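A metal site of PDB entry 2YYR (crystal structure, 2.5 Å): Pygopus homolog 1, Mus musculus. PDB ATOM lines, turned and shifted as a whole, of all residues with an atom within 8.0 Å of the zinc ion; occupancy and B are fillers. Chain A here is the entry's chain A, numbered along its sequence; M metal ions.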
ATOM      1  N   GLY A  13     -30.957   5.480   7.377  1.00  0.00           N
ATOM      2  CA  GLY A  13     -31.934   4.882   8.276  1.00  0.00           C
ATOM      3  C   GLY A  13     -33.380   5.274   8.038  1.00  0.00           C
ATOM      4  O   GLY A  13     -34.285   4.694   8.653  1.00  0.00           O
ATOM      5  N   LEU A  27     -24.404  10.459  11.770  1.00  0.00           N
ATOM      6  CA  LEU A  27     -24.392   9.131  12.360  1.00  0.00           C
ATOM      7  C   LEU A  27     -25.091   9.120  13.719  1.00  0.00           C
ATOM      8  O   LEU A  27     -24.892  10.021  14.526  1.00  0.00           O
ATOM      9  CB  LEU A  27     -22.949   8.663  12.529  1.00  0.00           C
ATOM     10  CG  LEU A  27     -22.662   7.293  13.161  1.00  0.00           C
ATOM     11  CD1 LEU A  27     -23.214   6.202  12.279  1.00  0.00           C
ATOM     12  CD2 LEU A  27     -21.161   7.124  13.337  1.00  0.00           C
ATOM     13  N   CYS A  28     -25.912   8.105  13.948  1.00  0.00           N
ATOM     14  CA  CYS A  28     -26.612   7.987  15.233  1.00  0.00           C
ATOM     15  C   CYS A  28     -25.676   7.313  16.222  1.00  0.00           C
ATOM     16  O   CYS A  28     -25.669   6.091  16.350  1.00  0.00           O
ATOM     17  CB  CYS A  28     -27.893   7.172  15.084  1.00  0.00           C
ATOM     18  SG  CYS A  28     -28.704   6.781  16.668  1.00  0.00           S
ATOM     19  N   GLU A  29     -24.854   8.120  16.891  1.00  0.00           N
ATOM     20  CA  GLU A  29     -23.895   7.607  17.868  1.00  0.00           C
ATOM     21  C   GLU A  29     -24.597   7.230  19.162  1.00  0.00           C
ATOM     22  O   GLU A  29     -24.011   6.604  20.043  1.00  0.00           O
ATOM     23  CB  GLU A  29     -22.793   8.627  18.126  1.00  0.00           C
ATOM     24  CG  GLU A  29     -21.946   8.908  16.892  1.00  0.00           C
ATOM     25  CD  GLU A  29     -20.837   9.917  17.148  1.00  0.00           C
ATOM     26  OE1 GLU A  29     -21.148  11.076  17.500  1.00  0.00           O
ATOM     27  OE2 GLU A  29     -19.652   9.545  16.965  1.00  0.00           O
ATOM     28  N   ALA A  30     -25.875   7.599  19.260  1.00  0.00           N
ATOM     29  CA  ALA A  30     -26.677   7.296  20.444  1.00  0.00           C
ATOM     30  C   ALA A  30     -26.895   5.797  20.604  1.00  0.00           C
ATOM     31  O   ALA A  30     -26.898   5.295  21.738  1.00  0.00           O
ATOM     32  CB  ALA A  30     -28.003   8.039  20.398  1.00  0.00           C
ATOM     33  N   SER A  31     -27.070   5.081  19.486  1.00  0.00           N
ATOM     34  CA  SER A  31     -27.293   3.643  19.573  1.00  0.00           C
ATOM     35  C   SER A  31     -27.109   2.810  18.298  1.00  0.00           C
ATOM     36  O   SER A  31     -26.111   2.098  18.161  1.00  0.00           O
ATOM     37  CB  SER A  31     -28.666   3.341  20.173  1.00  0.00           C
ATOM     38  OG  SER A  31     -28.883   1.945  20.287  1.00  0.00           O
ATOM     39  N   CYS A  32     -28.079   2.897  17.389  1.00  0.00           N
ATOM     40  CA  CYS A  32     -28.087   2.105  16.148  1.00  0.00           C
ATOM     41  C   CYS A  32     -26.882   2.193  15.209  1.00  0.00           C
ATOM     42  O   CYS A  32     -26.705   1.321  14.349  1.00  0.00           O
ATOM     43  CB  CYS A  32     -29.378   2.340  15.359  1.00  0.00           C
ATOM     44  SG  CYS A  32     -29.469   3.896  14.471  1.00  0.00           S
ATOM     45  N   GLN A  33     -26.071   3.233  15.351  1.00  0.00           N
ATOM     46  CA  GLN A  33     -24.882   3.421  14.522  1.00  0.00           C
ATOM     47  C   GLN A  33     -25.133   3.492  13.018  1.00  0.00           C
ATOM     48  O   GLN A  33     -24.258   3.175  12.221  1.00  0.00           O
ATOM     49  CB  GLN A  33     -23.839   2.335  14.827  1.00  0.00           C
ATOM     50  CG  GLN A  33     -23.272   2.370  16.247  1.00  0.00           C
ATOM     51  CD  GLN A  33     -22.567   3.676  16.577  1.00  0.00           C
ATOM     52  OE1 GLN A  33     -21.678   4.123  15.838  1.00  0.00           O
ATOM     53  NE2 GLN A  33     -22.953   4.296  17.687  1.00  0.00           N
ATOM     54  N   LYS A  34     -26.332   3.923  12.628  1.00  0.00           N
ATOM     55  CA  LYS A  34     -26.657   4.060  11.206  1.00  0.00           C
ATOM     56  C   LYS A  34     -26.584   5.527  10.772  1.00  0.00           C
ATOM     57  O   LYS A  34     -26.731   6.434  11.590  1.00  0.00           O
ATOM     58  CB  LYS A  34     -28.037   3.486  10.910  1.00  0.00           C
ATOM     59  CG  LYS A  34     -28.044   1.957  10.793  1.00  0.00           C
ATOM     60  CD  LYS A  34     -29.408   1.403  10.388  1.00  0.00           C
ATOM     61  CE  LYS A  34     -30.431   1.547  11.504  1.00  0.00           C
ATOM     62  NZ  LYS A  34     -31.719   0.873  11.195  1.00  0.00           N
ATOM     63  N   TRP A  35     -26.283   5.737   9.488  1.00  0.00           N
ATOM     64  CA  TRP A  35     -26.196   7.089   8.933  1.00  0.00           C
ATOM     65  C   TRP A  35     -27.568   7.562   8.499  1.00  0.00           C
ATOM     66  O   TRP A  35     -28.373   6.775   7.982  1.00  0.00           O
ATOM     67  CB  TRP A  35     -25.226   7.134   7.760  1.00  0.00           C
ATOM     68  CG  TRP A  35     -23.776   7.076   8.148  1.00  0.00           C
ATOM     69  CD1 TRP A  35     -22.993   5.964   8.215  1.00  0.00           C
ATOM     70  CD2 TRP A  35     -22.935   8.182   8.515  1.00  0.00           C
ATOM     71  NE1 TRP A  35     -21.710   6.303   8.580  1.00  0.00           N
ATOM     72  CE2 TRP A  35     -21.653   7.656   8.773  1.00  0.00           C
ATOM     73  CE3 TRP A  35     -23.149   9.561   8.634  1.00  0.00           C
ATOM     74  CZ2 TRP A  35     -20.571   8.464   9.160  1.00  0.00           C
ATOM     75  CZ3 TRP A  35     -22.077  10.364   9.013  1.00  0.00           C
ATOM     76  CH2 TRP A  35     -20.806   9.813   9.275  1.00  0.00           C
ATOM     77  N   PHE A  36     -27.856   8.843   8.713  1.00  0.00           N
ATOM     78  CA  PHE A  36     -29.141   9.420   8.339  1.00  0.00           C
ATOM     79  C   PHE A  36     -28.914  10.726   7.584  1.00  0.00           C
ATOM     80  O   PHE A  36     -28.233  11.615   8.082  1.00  0.00           O
ATOM     81  CB  PHE A  36     -29.976   9.738   9.589  1.00  0.00           C
ATOM     82  CG  PHE A  36     -30.368   8.516  10.381  1.00  0.00           C
ATOM     83  CD1 PHE A  36     -29.439   7.846  11.161  1.00  0.00           C
ATOM     84  CD2 PHE A  36     -31.680   8.061  10.350  1.00  0.00           C
ATOM     85  CE1 PHE A  36     -29.803   6.728  11.898  1.00  0.00           C
ATOM     86  CE2 PHE A  36     -32.067   6.937  11.083  1.00  0.00           C
ATOM     87  CZ  PHE A  36     -31.115   6.273  11.867  1.00  0.00           C
ATOM     88  N   TRP A  59     -25.437  12.711  18.669  1.00  0.00           N
ATOM     89  CA  TRP A  59     -26.786  12.716  18.118  1.00  0.00           C
ATOM     90  C   TRP A  59     -27.402  11.323  18.054  1.00  0.00           C
ATOM     91  O   TRP A  59     -26.704  10.336  17.852  1.00  0.00           O
ATOM     92  CB  TRP A  59     -26.756  13.348  16.723  1.00  0.00           C
ATOM     93  CG  TRP A  59     -28.102  13.385  16.049  1.00  0.00           C
ATOM     94  CD1 TRP A  59     -29.056  14.353  16.186  1.00  0.00           C
ATOM     95  CD2 TRP A  59     -28.625  12.451  15.103  1.00  0.00           C
ATOM     96  NE1 TRP A  59     -30.137  14.071  15.392  1.00  0.00           N
ATOM     97  CE2 TRP A  59     -29.898  12.902  14.718  1.00  0.00           C
ATOM     98  CE3 TRP A  59     -28.131  11.257  14.543  1.00  0.00           C
ATOM     99  CZ2 TRP A  59     -30.698  12.212  13.790  1.00  0.00           C
ATOM    100  CZ3 TRP A  59     -28.926  10.567  13.632  1.00  0.00           C
ATOM    101  CH2 TRP A  59     -30.190  11.056  13.260  1.00  0.00           C
ATOM    102  N   GLY A  60     -28.730  11.287  18.195  1.00  0.00           N
ATOM    103  CA  GLY A  60     -29.460  10.033  18.125  1.00  0.00           C
ATOM    104  C   GLY A  60     -30.721  10.184  17.293  1.00  0.00           C
ATOM    105  O   GLY A  60     -31.391  11.219  17.357  1.00  0.00           O
ATOM    106  N   CYS A  61     -31.042   9.159  16.499  1.00  0.00           N
ATOM    107  CA  CYS A  61     -32.223   9.197  15.640  1.00  0.00           C
ATOM    108  C   CYS A  61     -33.516   9.091  16.438  1.00  0.00           C
ATOM    109  O   CYS A  61     -33.517   8.638  17.587  1.00  0.00           O
ATOM    110  CB  CYS A  61     -32.163   8.076  14.596  1.00  0.00           C
ATOM    111  SG  CYS A  61     -32.295   6.411  15.274  1.00  0.00           S
ATOM    112  N   ASP A  62     -34.637   9.492  15.819  1.00  0.00           N
ATOM    113  CA  ASP A  62     -35.938   9.450  16.466  1.00  0.00           C
ATOM    114  C   ASP A  62     -36.296   8.062  17.005  1.00  0.00           C
ATOM    115  O   ASP A  62     -36.941   7.952  18.042  1.00  0.00           O
ATOM    116  CB  ASP A  62     -37.030   9.934  15.508  1.00  0.00           C
ATOM    117  CG  ASP A  62     -36.915  11.418  15.187  1.00  0.00           C
ATOM    118  OD1 ASP A  62     -37.047  11.784  13.998  1.00  0.00           O
ATOM    119  OD2 ASP A  62     -36.687  12.225  16.116  1.00  0.00           O
ATOM    120  N   THR A  63     -35.848   7.023  16.309  1.00  0.00           N
ATOM    121  CA  THR A  63     -36.097   5.641  16.722  1.00  0.00           C
ATOM    122  C   THR A  63     -35.365   5.318  18.030  1.00  0.00           C
ATOM    123  O   THR A  63     -35.977   4.861  18.984  1.00  0.00           O
ATOM    124  CB  THR A  63     -35.664   4.639  15.636  1.00  0.00           C
ATOM    125  OG1 THR A  63     -36.514   4.793  14.486  1.00  0.00           O
ATOM    126  CG2 THR A  63     -35.755   3.200  16.141  1.00  0.00           C
ATOM    127  N   CYS A  64     -34.067   5.587  18.054  1.00  0.00           N
ATOM    128  CA  CYS A  64     -33.250   5.329  19.242  1.00  0.00           C
ATOM    129  C   CYS A  64     -33.605   6.240  20.416  1.00  0.00           C
ATOM    130  O   CYS A  64     -33.604   5.795  21.571  1.00  0.00           O
ATOM    131  CB  CYS A  64     -31.774   5.458  18.906  1.00  0.00           C
ATOM    132  SG  CYS A  64     -31.179   4.205  17.765  1.00  0.00           S
ATOM    133  N   MET A  65     -33.924   7.499  20.131  1.00  0.00           N
ATOM    134  CA  MET A  65     -34.273   8.448  21.188  1.00  0.00           C
ATOM    135  C   MET A  65     -35.615   8.133  21.839  1.00  0.00           C
ATOM    136  O   MET A  65     -35.849   8.494  23.002  1.00  0.00           O
ATOM    137  CB  MET A  65     -34.265   9.889  20.660  1.00  0.00           C
ATOM    138  CG  MET A  65     -32.887  10.370  20.227  1.00  0.00           C
ATOM    139  SD  MET A  65     -31.485  10.007  21.507  1.00  0.00           S
ATOM    140  CE  MET A  65     -31.864  11.412  22.774  1.00  0.00           C
HETATM  141 ZN    ZN M   1     -30.427   5.345  15.888  1.00  0.00          ZN
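Four residues have an atom within 4 Å of the zinc ion: Cys 28, Cys 32, Cys 61 and Cys 64. The nearest printed residue that does not touch the zinc ion is Phe 36 (4.2 Å).
SG of Cys 61 sits close to N of Thr 63 (3.8 Å). SG of Cys 32 lies close to N of Lys 34 (3.6 Å). SG of Cys 28 sits close to N of Ser 31, 3.7 Å away. N of Gln 33 is in hydrogen-bond range of O of Cys 28, 3.1 Å away. The backbone NH of Cys 28 sits at hydrogen-bond distance from the backbone carbonyl oxygen of Lys 34 (3.0 Å).
The zinc ion is bound by SG of Cys 61, 2.2 Å away. SG of Cys 32 binds the zinc ion, 2.2 Å away. SG of Cys 64 is bound to the zinc ion, 2.3 Å away. The side-chain sulfur (SG) of Cys 28 binds the zinc ion (2.4 Å). The zinc ion has four donor atoms within binding distance.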
